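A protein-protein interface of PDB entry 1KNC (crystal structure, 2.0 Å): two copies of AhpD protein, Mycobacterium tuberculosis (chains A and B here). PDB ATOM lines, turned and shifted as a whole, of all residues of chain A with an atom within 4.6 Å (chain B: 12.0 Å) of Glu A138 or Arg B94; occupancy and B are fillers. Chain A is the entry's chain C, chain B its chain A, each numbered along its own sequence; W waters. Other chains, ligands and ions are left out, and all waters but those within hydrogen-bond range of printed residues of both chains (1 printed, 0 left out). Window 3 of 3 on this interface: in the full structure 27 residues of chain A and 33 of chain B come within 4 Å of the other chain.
The guanidinium group (NE) of Arg B94 lies close to the backbone carbonyl oxygen (O) of Leu B91 (3.3 Å).
OE2 of Glu A138 is in salt-bridge range of NH1 of Arg A142 (3.0 Å).
No position is printed for both chains.
The side-chain carboxylate (OE1) of Glu A138 is in salt-bridge range of the guanidinium group (NH1) of Arg B94, 3.3 Å away.
The backbone carbonyl oxygen of Arg B94 is in hydrogen-bond range of the guanidinium group of Arg A148.
The side-chain hydroxyl of Tyr B95 lies within hydrogen-bond range of the side-chain carboxylate of Glu A138, 2.5 Å away.
The guanidinium group (NH2) of Arg A148 lies within salt-bridge range of the side-chain carboxylate (OD1) of Asp B97, 2.6 Å away.
Among the printed residues, merely in contact across the chains: Val A135 with Phe B90, Ile A151 with Tyr B95, Leu A134 with Leu B91, Arg A148 with Tyr B95, Arg A148 with Leu B98, Glu A138 with Leu B91, Leu A134 with Gly B87 and Arg A142 with Tyr B95.
No residue of chain B comes within 4 Å of Phe A122.
Of the printed residues of chain B, Leu A134 touches Gly B87 and Leu B91.
Val A135 touches just one residue of chain B: Phe B90.
No residue of chain B comes within 4 Å of Ala A136.
No residue of chain B comes within 4 Å of His A137.
Glu A138 touches just these residues of chain B: Leu B91 (3.8 Å), Arg B94 (3.3 Å) and Tyr B95 (2.5 Å).
No residue of chain B comes within 4 Å of His A139.
No residue of chain B comes within 4 Å of Thr A140.
No residue of chain B comes within 4 Å of Leu A141.
Arg A142 touches just one residue of chain B: Tyr B95 (3.8 Å).
Of chain B, only Arg B94 (2.9 Å), Tyr B95 (3.5 Å), Asp B97 (2.6 Å) and Leu B98 (3.6 Å) come within 4 Å of Arg A148.
Of chain B, only Tyr B95 (3.5 Å) comes within 4 Å of Ile A151.
Printed residues of chain A within 4 Å of Gly B87: Leu A134 (3.8 Å).
Of the printed residues of chain A, Leu B91 touches Leu A134 and Glu A138.
Arg B94 touches just these residues of chain A: Glu A138 and Arg A148.
Printed residues of chain A within 4 Å of Leu B98: Arg A148.
The nearest residue of chain A that does not touch Arg B94 is Val A135 (4.2 Å).
The nearest printed residue of chain A that does not touch Asp B97 is Arg A142 (9.0 Å).
Water W1 lies within hydrogen-bond range of the backbone carbonyl oxygen (O) of Val A135 (2.6 Å), the side-chain carboxylate (OE1) of Glu A138 (2.6 Å), the guanidinium group (NH2) of Arg B94 (2.8 Å) and the backbone NH (N) of His A139 (3.5 Å).
Of the 12 printed residues of chain A, 6 touch a printed residue of chain B.
Printed residues of chain A that touch a printed residue of chain B: Leu A134, Val A135, Glu A138, Arg A142, Arg A148 and Ile A151.
Hydrophobic or aromatic side chains of chain A that line the printed part of chain B: Leu A134, Val A135 and Ile A151.
Of the 18 printed residues of chain B, 7 touch a printed residue of chain A.
Printed residues of chain B that touch a printed residue of chain A: Gly B87, Phe B90, Leu B91, Arg B94, Tyr B95, Asp B97 and Leu B98.
Hydrophobic or aromatic side chains of chain B that line the printed part of chain A: Leu B91, Tyr B95 and Leu B98.
Among the printed residues, 12 pairs touch across the chains.
Among the printed residues, Asp or Glu carboxylates within 4 Å of a Lys or Arg side-chain nitrogen of the other chain: Glu A138 with Arg B94 and Arg A148 with Asp B97.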
ATOM      1  N   PHE A 122       3.005  -4.830 -20.834  1.00  0.00           N
ATOM      2  CA  PHE A 122       1.811  -5.657 -20.952  1.00  0.00           C
ATOM      3  C   PHE A 122       1.831  -6.259 -22.353  1.00  0.00           C
ATOM      4  O   PHE A 122       1.638  -7.461 -22.532  1.00  0.00           O
ATOM      5  CB  PHE A 122       0.552  -4.797 -20.780  1.00  0.00           C
ATOM      6  CG  PHE A 122      -0.724  -5.489 -21.195  1.00  0.00           C
ATOM      7  CD1 PHE A 122      -1.379  -6.359 -20.335  1.00  0.00           C
ATOM      8  CD2 PHE A 122      -1.265  -5.260 -22.454  1.00  0.00           C
ATOM      9  CE1 PHE A 122      -2.564  -6.992 -20.728  1.00  0.00           C
ATOM     10  CE2 PHE A 122      -2.446  -5.887 -22.859  1.00  0.00           C
ATOM     11  CZ  PHE A 122      -3.093  -6.752 -21.992  1.00  0.00           C
ATOM     12  N   LEU A 134       1.527 -10.571 -17.580  1.00  0.00           N
ATOM     13  CA  LEU A 134       0.450  -9.883 -18.261  1.00  0.00           C
ATOM     14  C   LEU A 134      -0.605  -9.468 -17.235  1.00  0.00           C
ATOM     15  O   LEU A 134      -1.020  -8.306 -17.197  1.00  0.00           O
ATOM     16  CB  LEU A 134      -0.151 -10.773 -19.351  1.00  0.00           C
ATOM     17  CG  LEU A 134      -1.177 -10.031 -20.216  1.00  0.00           C
ATOM     18  CD1 LEU A 134      -1.001 -10.375 -21.681  1.00  0.00           C
ATOM     19  CD2 LEU A 134      -2.572 -10.401 -19.720  1.00  0.00           C
ATOM     20  N   VAL A 135      -1.008 -10.403 -16.383  1.00  0.00           N
ATOM     21  CA  VAL A 135      -2.003 -10.110 -15.357  1.00  0.00           C
ATOM     22  C   VAL A 135      -1.512  -9.043 -14.377  1.00  0.00           C
ATOM     23  O   VAL A 135      -2.291  -8.192 -13.942  1.00  0.00           O
ATOM     24  CB  VAL A 135      -2.397 -11.384 -14.576  1.00  0.00           C
ATOM     25  CG1 VAL A 135      -3.385 -11.037 -13.464  1.00  0.00           C
ATOM     26  CG2 VAL A 135      -3.024 -12.396 -15.530  1.00  0.00           C
ATOM     27  N   ALA A 136      -0.225  -9.071 -14.036  1.00  0.00           N
ATOM     28  CA  ALA A 136       0.322  -8.082 -13.102  1.00  0.00           C
ATOM     29  C   ALA A 136       0.303  -6.678 -13.701  1.00  0.00           C
ATOM     30  O   ALA A 136      -0.150  -5.723 -13.065  1.00  0.00           O
ATOM     31  CB  ALA A 136       1.751  -8.453 -12.700  1.00  0.00           C
ATOM     32  N   HIS A 137       0.790  -6.555 -14.928  1.00  0.00           N
ATOM     33  CA  HIS A 137       0.816  -5.258 -15.576  1.00  0.00           C
ATOM     34  C   HIS A 137      -0.580  -4.741 -15.920  1.00  0.00           C
ATOM     35  O   HIS A 137      -0.802  -3.529 -15.976  1.00  0.00           O
ATOM     36  CB  HIS A 137       1.689  -5.321 -16.824  1.00  0.00           C
ATOM     37  CG  HIS A 137       3.120  -5.660 -16.533  1.00  0.00           C
ATOM     38  ND1 HIS A 137       3.903  -4.912 -15.680  1.00  0.00           N
ATOM     39  CD2 HIS A 137       3.910  -6.662 -16.986  1.00  0.00           C
ATOM     40  CE1 HIS A 137       5.115  -5.437 -15.622  1.00  0.00           C
ATOM     41  NE2 HIS A 137       5.145  -6.498 -16.406  1.00  0.00           N
ATOM     42  N   GLU A 138      -1.522  -5.652 -16.145  1.00  0.00           N
ATOM     43  CA  GLU A 138      -2.889  -5.256 -16.460  1.00  0.00           C
ATOM     44  C   GLU A 138      -3.478  -4.578 -15.230  1.00  0.00           C
ATOM     45  O   GLU A 138      -4.068  -3.504 -15.330  1.00  0.00           O
ATOM     46  CB  GLU A 138      -3.727  -6.483 -16.827  1.00  0.00           C
ATOM     47  CG  GLU A 138      -5.091  -6.173 -17.445  1.00  0.00           C
ATOM     48  CD  GLU A 138      -6.170  -5.858 -16.420  1.00  0.00           C
ATOM     49  OE1 GLU A 138      -6.065  -6.332 -15.266  1.00  0.00           O
ATOM     50  OE2 GLU A 138      -7.139  -5.151 -16.783  1.00  0.00           O
ATOM     51  N   HIS A 139      -3.304  -5.210 -14.072  1.00  0.00           N
ATOM     52  CA  HIS A 139      -3.819  -4.666 -12.823  1.00  0.00           C
ATOM     53  C   HIS A 139      -3.219  -3.288 -12.535  1.00  0.00           C
ATOM     54  O   HIS A 139      -3.932  -2.358 -12.157  1.00  0.00           O
ATOM     55  CB  HIS A 139      -3.518  -5.617 -11.659  1.00  0.00           C
ATOM     56  CG  HIS A 139      -4.188  -5.227 -10.378  1.00  0.00           C
ATOM     57  ND1 HIS A 139      -5.555  -5.281 -10.207  1.00  0.00           N
ATOM     58  CD2 HIS A 139      -3.683  -4.755  -9.214  1.00  0.00           C
ATOM     59  CE1 HIS A 139      -5.864  -4.859  -8.994  1.00  0.00           C
ATOM     60  NE2 HIS A 139      -4.746  -4.533  -8.370  1.00  0.00           N
ATOM     61  N   THR A 140      -1.910  -3.161 -12.723  1.00  0.00           N
ATOM     62  CA  THR A 140      -1.219  -1.895 -12.488  1.00  0.00           C
ATOM     63  C   THR A 140      -1.766  -0.785 -13.386  1.00  0.00           C
ATOM     64  O   THR A 140      -1.967   0.343 -12.937  1.00  0.00           O
ATOM     65  CB  THR A 140       0.304  -2.049 -12.719  1.00  0.00           C
ATOM     66  OG1 THR A 140       0.828  -2.994 -11.776  1.00  0.00           O
ATOM     67  CG2 THR A 140       1.016  -0.714 -12.543  1.00  0.00           C
ATOM     68  N   LEU A 141      -2.005  -1.107 -14.653  1.00  0.00           N
ATOM     69  CA  LEU A 141      -2.540  -0.130 -15.590  1.00  0.00           C
ATOM     70  C   LEU A 141      -3.942   0.306 -15.159  1.00  0.00           C
ATOM     71  O   LEU A 141      -4.296   1.479 -15.273  1.00  0.00           O
ATOM     72  CB  LEU A 141      -2.588  -0.718 -17.003  1.00  0.00           C
ATOM     73  CG  LEU A 141      -1.225  -0.853 -17.688  1.00  0.00           C
ATOM     74  CD1 LEU A 141      -1.294  -1.898 -18.787  1.00  0.00           C
ATOM     75  CD2 LEU A 141      -0.793   0.493 -18.236  1.00  0.00           C
ATOM     76  N   ARG A 142      -4.732  -0.637 -14.660  1.00  0.00           N
ATOM     77  CA  ARG A 142      -6.082  -0.324 -14.217  1.00  0.00           C
ATOM     78  C   ARG A 142      -6.082   0.531 -12.955  1.00  0.00           C
ATOM     79  O   ARG A 142      -7.033   1.268 -12.702  1.00  0.00           O
ATOM     80  CB  ARG A 142      -6.885  -1.608 -13.972  1.00  0.00           C
ATOM     81  CG  ARG A 142      -7.263  -2.358 -15.248  1.00  0.00           C
ATOM     82  CD  ARG A 142      -8.326  -1.617 -16.056  1.00  0.00           C
ATOM     83  NE  ARG A 142      -9.658  -1.753 -15.468  1.00  0.00           N
ATOM     84  CZ  ARG A 142     -10.326  -2.900 -15.377  1.00  0.00           C
ATOM     85  NH1 ARG A 142      -9.786  -4.021 -15.843  1.00  0.00           N
ATOM     86  NH2 ARG A 142     -11.532  -2.929 -14.822  1.00  0.00           N
ATOM     87  N   ARG A 148      -9.876  -0.357 -19.906  1.00  0.00           N
ATOM     88  CA  ARG A 148      -9.726  -1.685 -20.495  1.00  0.00           C
ATOM     89  C   ARG A 148      -9.620  -1.555 -22.010  1.00  0.00           C
ATOM     90  O   ARG A 148      -8.876  -2.294 -22.659  1.00  0.00           O
ATOM     91  CB  ARG A 148     -10.922  -2.568 -20.141  1.00  0.00           C
ATOM     92  CG  ARG A 148     -11.040  -2.868 -18.670  1.00  0.00           C
ATOM     93  CD  ARG A 148     -12.406  -3.433 -18.355  1.00  0.00           C
ATOM     94  NE  ARG A 148     -12.689  -4.622 -19.138  1.00  0.00           N
ATOM     95  CZ  ARG A 148     -13.709  -4.740 -19.985  1.00  0.00           C
ATOM     96  NH1 ARG A 148     -14.555  -3.738 -20.168  1.00  0.00           N
ATOM     97  NH2 ARG A 148     -13.877  -5.867 -20.664  1.00  0.00           N
ATOM     98  N   ILE A 151      -6.068  -0.815 -22.849  1.00  0.00           N
ATOM     99  CA  ILE A 151      -5.228  -1.984 -22.636  1.00  0.00           C
ATOM    100  C   ILE A 151      -5.506  -2.982 -23.759  1.00  0.00           C
ATOM    101  O   ILE A 151      -4.588  -3.573 -24.332  1.00  0.00           O
ATOM    102  CB  ILE A 151      -5.536  -2.605 -21.272  1.00  0.00           C
ATOM    103  CG1 ILE A 151      -5.178  -1.596 -20.177  1.00  0.00           C
ATOM    104  CG2 ILE A 151      -4.739  -3.888 -21.073  1.00  0.00           C
ATOM    105  CD1 ILE A 151      -5.720  -1.962 -18.823  1.00  0.00           C
ATOM    106  N   PHE B  84      -3.103 -12.668 -29.652  1.00  0.00           N
ATOM    107  CA  PHE B  84      -4.335 -12.030 -29.187  1.00  0.00           C
ATOM    108  C   PHE B  84      -5.152 -12.889 -28.237  1.00  0.00           C
ATOM    109  O   PHE B  84      -5.496 -12.457 -27.134  1.00  0.00           O
ATOM    110  CB  PHE B  84      -5.237 -11.628 -30.364  1.00  0.00           C
ATOM    111  CG  PHE B  84      -6.579 -11.080 -29.927  1.00  0.00           C
ATOM    112  CD1 PHE B  84      -6.701  -9.762 -29.491  1.00  0.00           C
ATOM    113  CD2 PHE B  84      -7.699 -11.908 -29.876  1.00  0.00           C
ATOM    114  CE1 PHE B  84      -7.916  -9.276 -29.006  1.00  0.00           C
ATOM    115  CE2 PHE B  84      -8.922 -11.434 -29.391  1.00  0.00           C
ATOM    116  CZ  PHE B  84      -9.028 -10.113 -28.954  1.00  0.00           C
ATOM    117  N   TYR B  85      -5.482 -14.102 -28.664  1.00  0.00           N
ATOM    118  CA  TYR B  85      -6.280 -14.989 -27.835  1.00  0.00           C
ATOM    119  C   TYR B  85      -5.539 -15.531 -26.629  1.00  0.00           C
ATOM    120  O   TYR B  85      -6.152 -15.879 -25.618  1.00  0.00           O
ATOM    121  CB  TYR B  85      -6.824 -16.137 -28.675  1.00  0.00           C
ATOM    122  CG  TYR B  85      -7.937 -15.691 -29.592  1.00  0.00           C
ATOM    123  CD1 TYR B  85      -9.175 -15.306 -29.075  1.00  0.00           C
ATOM    124  CD2 TYR B  85      -7.739 -15.597 -30.970  1.00  0.00           C
ATOM    125  CE1 TYR B  85     -10.184 -14.833 -29.900  1.00  0.00           C
ATOM    126  CE2 TYR B  85      -8.741 -15.125 -31.804  1.00  0.00           C
ATOM    127  CZ  TYR B  85      -9.963 -14.744 -31.260  1.00  0.00           C
ATOM    128  OH  TYR B  85     -10.941 -14.271 -32.094  1.00  0.00           O
ATOM    129  N   ARG B  86      -4.219 -15.623 -26.726  1.00  0.00           N
ATOM    130  CA  ARG B  86      -3.441 -16.113 -25.591  1.00  0.00           C
ATOM    131  C   ARG B  86      -3.482 -15.054 -24.487  1.00  0.00           C
ATOM    132  O   ARG B  86      -3.746 -15.363 -23.323  1.00  0.00           O
ATOM    133  CB  ARG B  86      -1.982 -16.391 -26.003  1.00  0.00           C
ATOM    134  CG  ARG B  86      -1.053 -16.749 -24.836  1.00  0.00           C
ATOM    135  CD  ARG B  86       0.312 -17.240 -25.330  1.00  0.00           C
ATOM    136  NE  ARG B  86       1.090 -16.178 -25.953  1.00  0.00           N
ATOM    137  CZ  ARG B  86       1.809 -16.323 -27.061  1.00  0.00           C
ATOM    138  NH1 ARG B  86       1.851 -17.497 -27.677  1.00  0.00           N
ATOM    139  NH2 ARG B  86       2.478 -15.289 -27.560  1.00  0.00           N
ATOM    140  N   GLY B  87      -3.220 -13.809 -24.867  1.00  0.00           N
ATOM    141  CA  GLY B  87      -3.236 -12.720 -23.909  1.00  0.00           C
ATOM    142  C   GLY B  87      -4.607 -12.576 -23.283  1.00  0.00           C
ATOM    143  O   GLY B  87      -4.738 -12.451 -22.067  1.00  0.00           O
ATOM    144  N   ARG B  88      -5.638 -12.603 -24.123  1.00  0.00           N
ATOM    145  CA  ARG B  88      -7.012 -12.481 -23.647  1.00  0.00           C
ATOM    146  C   ARG B  88      -7.331 -13.629 -22.700  1.00  0.00           C
ATOM    147  O   ARG B  88      -8.033 -13.463 -21.696  1.00  0.00           O
ATOM    148  CB  ARG B  88      -7.982 -12.505 -24.826  1.00  0.00           C
ATOM    149  CG  ARG B  88      -9.426 -12.287 -24.424  1.00  0.00           C
ATOM    150  CD  ARG B  88     -10.336 -12.281 -25.626  1.00  0.00           C
ATOM    151  NE  ARG B  88     -10.823 -13.619 -25.934  1.00  0.00           N
ATOM    152  CZ  ARG B  88     -11.895 -13.867 -26.675  1.00  0.00           C
ATOM    153  NH1 ARG B  88     -12.596 -12.865 -27.193  1.00  0.00           N
ATOM    154  NH2 ARG B  88     -12.277 -15.118 -26.869  1.00  0.00           N
ATOM    155  N   GLY B  89      -6.800 -14.801 -23.029  1.00  0.00           N
ATOM    156  CA  GLY B  89      -7.024 -15.979 -22.208  1.00  0.00           C
ATOM    157  C   GLY B  89      -6.474 -15.848 -20.797  1.00  0.00           C
ATOM    158  O   GLY B  89      -7.084 -16.325 -19.837  1.00  0.00           O
ATOM    159  N   PHE B  90      -5.316 -15.210 -20.665  1.00  0.00           N
ATOM    160  CA  PHE B  90      -4.707 -15.024 -19.353  1.00  0.00           C
ATOM    161  C   PHE B  90      -5.558 -14.130 -18.458  1.00  0.00           C
ATOM    162  O   PHE B  90      -5.422 -14.155 -17.237  1.00  0.00           O
ATOM    163  CB  PHE B  90      -3.306 -14.405 -19.485  1.00  0.00           C
ATOM    164  CG  PHE B  90      -2.289 -15.319 -20.121  1.00  0.00           C
ATOM    165  CD1 PHE B  90      -2.369 -16.696 -19.951  1.00  0.00           C
ATOM    166  CD2 PHE B  90      -1.226 -14.794 -20.852  1.00  0.00           C
ATOM    167  CE1 PHE B  90      -1.402 -17.545 -20.498  1.00  0.00           C
ATOM    168  CE2 PHE B  90      -0.250 -15.633 -21.403  1.00  0.00           C
ATOM    169  CZ  PHE B  90      -0.343 -17.009 -21.222  1.00  0.00           C
ATOM    170  N   LEU B  91      -6.435 -13.338 -19.068  1.00  0.00           N
ATOM    171  CA  LEU B  91      -7.293 -12.426 -18.310  1.00  0.00           C
ATOM    172  C   LEU B  91      -8.573 -13.102 -17.821  1.00  0.00           C
ATOM    173  O   LEU B  91      -9.480 -12.447 -17.300  1.00  0.00           O
ATOM    174  CB  LEU B  91      -7.611 -11.194 -19.160  1.00  0.00           C
ATOM    175  CG  LEU B  91      -6.353 -10.419 -19.569  1.00  0.00           C
ATOM    176  CD1 LEU B  91      -6.688  -9.368 -20.610  1.00  0.00           C
ATOM    177  CD2 LEU B  91      -5.719  -9.780 -18.338  1.00  0.00           C
ATOM    178  N   GLU B  92      -8.635 -14.418 -18.002  1.00  0.00           N
ATOM    179  CA  GLU B  92      -9.763 -15.226 -17.552  1.00  0.00           C
ATOM    180  C   GLU B  92     -11.150 -14.728 -17.955  1.00  0.00           C
ATOM    181  O   GLU B  92     -12.068 -14.721 -17.137  1.00  0.00           O
ATOM    182  CB  GLU B  92      -9.730 -15.371 -16.026  1.00  0.00           C
ATOM    183  CG  GLU B  92      -8.425 -15.918 -15.441  1.00  0.00           C
ATOM    184  CD  GLU B  92      -8.074 -17.307 -15.943  1.00  0.00           C
ATOM    185  OE1 GLU B  92      -8.911 -18.232 -15.825  1.00  0.00           O
ATOM    186  OE2 GLU B  92      -6.947 -17.480 -16.452  1.00  0.00           O
ATOM    187  N   GLY B  93     -11.307 -14.313 -19.205  1.00  0.00           N
ATOM    188  CA  GLY B  93     -12.607 -13.855 -19.662  1.00  0.00           C
ATOM    189  C   GLY B  93     -12.984 -12.424 -19.327  1.00  0.00           C
ATOM    190  O   GLY B  93     -14.008 -11.932 -19.791  1.00  0.00           O
ATOM    191  N   ARG B  94     -12.166 -11.743 -18.532  1.00  0.00           N
ATOM    192  CA  ARG B  94     -12.470 -10.367 -18.170  1.00  0.00           C
ATOM    193  C   ARG B  94     -12.478  -9.438 -19.377  1.00  0.00           C
ATOM    194  O   ARG B  94     -13.010  -8.330 -19.314  1.00  0.00           O
ATOM    195  CB  ARG B  94     -11.488  -9.882 -17.102  1.00  0.00           C
ATOM    196  CG  ARG B  94     -11.614 -10.682 -15.804  1.00  0.00           C
ATOM    197  CD  ARG B  94     -10.820 -10.084 -14.658  1.00  0.00           C
ATOM    198  NE  ARG B  94      -9.392 -10.369 -14.757  1.00  0.00           N
ATOM    199  CZ  ARG B  94      -8.441  -9.440 -14.741  1.00  0.00           C
ATOM    200  NH1 ARG B  94      -8.771  -8.161 -14.636  1.00  0.00           N
ATOM    201  NH2 ARG B  94      -7.162  -9.792 -14.807  1.00  0.00           N
ATOM    202  N   TYR B  95     -11.902  -9.887 -20.488  1.00  0.00           N
ATOM    203  CA  TYR B  95     -11.890  -9.069 -21.700  1.00  0.00           C
ATOM    204  C   TYR B  95     -12.634  -9.731 -22.865  1.00  0.00           C
ATOM    205  O   TYR B  95     -12.536  -9.292 -24.005  1.00  0.00           O
ATOM    206  CB  TYR B  95     -10.449  -8.755 -22.109  1.00  0.00           C
ATOM    207  CG  TYR B  95      -9.798  -7.649 -21.299  1.00  0.00           C
ATOM    208  CD1 TYR B  95      -9.609  -7.776 -19.918  1.00  0.00           C
ATOM    209  CD2 TYR B  95      -9.351  -6.484 -21.922  1.00  0.00           C
ATOM    210  CE1 TYR B  95      -8.981  -6.764 -19.179  1.00  0.00           C
ATOM    211  CE2 TYR B  95      -8.728  -5.472 -21.199  1.00  0.00           C
ATOM    212  CZ  TYR B  95      -8.543  -5.618 -19.829  1.00  0.00           C
ATOM    213  OH  TYR B  95      -7.904  -4.622 -19.126  1.00  0.00           O
ATOM    214  N   ASP B  96     -13.386 -10.783 -22.563  1.00  0.00           N
ATOM    215  CA  ASP B  96     -14.135 -11.527 -23.572  1.00  0.00           C
ATOM    216  C   ASP B  96     -15.368 -10.812 -24.144  1.00  0.00           C
ATOM    217  O   ASP B  96     -15.945 -11.263 -25.135  1.00  0.00           O
ATOM    218  CB  ASP B  96     -14.546 -12.875 -22.993  1.00  0.00           C
ATOM    219  CG  ASP B  96     -13.395 -13.884 -22.984  1.00  0.00           C
ATOM    220  OD1 ASP B  96     -12.225 -13.471 -23.103  1.00  0.00           O
ATOM    221  OD2 ASP B  96     -13.673 -15.085 -22.844  1.00  0.00           O
ATOM    222  N   ASP B  97     -15.758  -9.694 -23.533  1.00  0.00           N
ATOM    223  CA  ASP B  97     -16.923  -8.937 -23.992  1.00  0.00           C
ATOM    224  C   ASP B  97     -16.554  -8.000 -25.129  1.00  0.00           C
ATOM    225  O   ASP B  97     -17.365  -7.718 -26.011  1.00  0.00           O
ATOM    226  CB  ASP B  97     -17.516  -8.133 -22.826  1.00  0.00           C
ATOM    227  CG  ASP B  97     -16.503  -7.194 -22.181  1.00  0.00           C
ATOM    228  OD1 ASP B  97     -15.427  -7.671 -21.770  1.00  0.00           O
ATOM    229  OD2 ASP B  97     -16.781  -5.981 -22.077  1.00  0.00           O
ATOM    230  N   LEU B  98     -15.309  -7.538 -25.118  1.00  0.00           N
ATOM    231  CA  LEU B  98     -14.835  -6.605 -26.129  1.00  0.00           C
ATOM    232  C   LEU B  98     -14.695  -7.228 -27.520  1.00  0.00           C
ATOM    233  O   LEU B  98     -14.318  -8.393 -27.664  1.00  0.00           O
ATOM    234  CB  LEU B  98     -13.504  -5.993 -25.667  1.00  0.00           C
ATOM    235  CG  LEU B  98     -13.535  -5.426 -24.234  1.00  0.00           C
ATOM    236  CD1 LEU B  98     -12.171  -4.884 -23.860  1.00  0.00           C
ATOM    237  CD2 LEU B  98     -14.591  -4.323 -24.115  1.00  0.00           C
ATOM    238  N   ARG B  99     -15.012  -6.431 -28.536  1.00  0.00           N
ATOM    239  CA  ARG B  99     -14.947  -6.863 -29.923  1.00  0.00           C
ATOM    240  C   ARG B  99     -13.504  -6.777 -30.410  1.00  0.00           C
ATOM    241  O   ARG B  99     -12.915  -5.696 -30.432  1.00  0.00           O
ATOM    242  CB  ARG B  99     -15.819  -5.955 -30.789  1.00  0.00           C
ATOM    243  CG  ARG B  99     -17.149  -5.612 -30.156  1.00  0.00           C
ATOM    244  CD  ARG B  99     -18.271  -6.292 -30.885  1.00  0.00           C
ATOM    245  NE  ARG B  99     -18.193  -6.054 -32.327  1.00  0.00           N
ATOM    246  CZ  ARG B  99     -19.017  -6.608 -33.208  1.00  0.00           C
ATOM    247  NH1 ARG B  99     -19.976  -7.420 -32.787  1.00  0.00           N
ATOM    248  NH2 ARG B  99     -18.872  -6.366 -34.501  1.00  0.00           N
ATOM    249  N   PRO B 100     -12.921  -7.920 -30.812  1.00  0.00           N
ATOM    250  CA  PRO B 100     -11.537  -7.941 -31.293  1.00  0.00           C
ATOM    251  C   PRO B 100     -11.286  -6.936 -32.403  1.00  0.00           C
ATOM    252  O   PRO B 100     -10.293  -6.213 -32.381  1.00  0.00           O
ATOM    253  CB  PRO B 100     -11.360  -9.381 -31.758  1.00  0.00           C
ATOM    254  CG  PRO B 100     -12.252 -10.142 -30.818  1.00  0.00           C
ATOM    255  CD  PRO B 100     -13.492  -9.279 -30.789  1.00  0.00           C
ATOM    256  N   HIS B 132      -6.087 -21.386 -26.216  1.00  0.00           N
ATOM    257  CA  HIS B 132      -7.371 -21.037 -26.816  1.00  0.00           C
ATOM    258  C   HIS B 132      -7.489 -21.490 -28.273  1.00  0.00           C
ATOM    259  O   HIS B 132      -8.414 -22.211 -28.634  1.00  0.00           O
ATOM    260  CB  HIS B 132      -7.623 -19.529 -26.727  1.00  0.00           C
ATOM    261  CG  HIS B 132      -8.938 -19.110 -27.304  1.00  0.00           C
ATOM    262  ND1 HIS B 132      -9.100 -18.779 -28.635  1.00  0.00           N
ATOM    263  CD2 HIS B 132     -10.167 -19.017 -26.747  1.00  0.00           C
ATOM    264  CE1 HIS B 132     -10.367 -18.499 -28.868  1.00  0.00           C
ATOM    265  NE2 HIS B 132     -11.039 -18.637 -27.737  1.00  0.00           N
HETATM  266  O   HOH W   1      -4.840  -8.313 -14.180  1.00  0.00           O
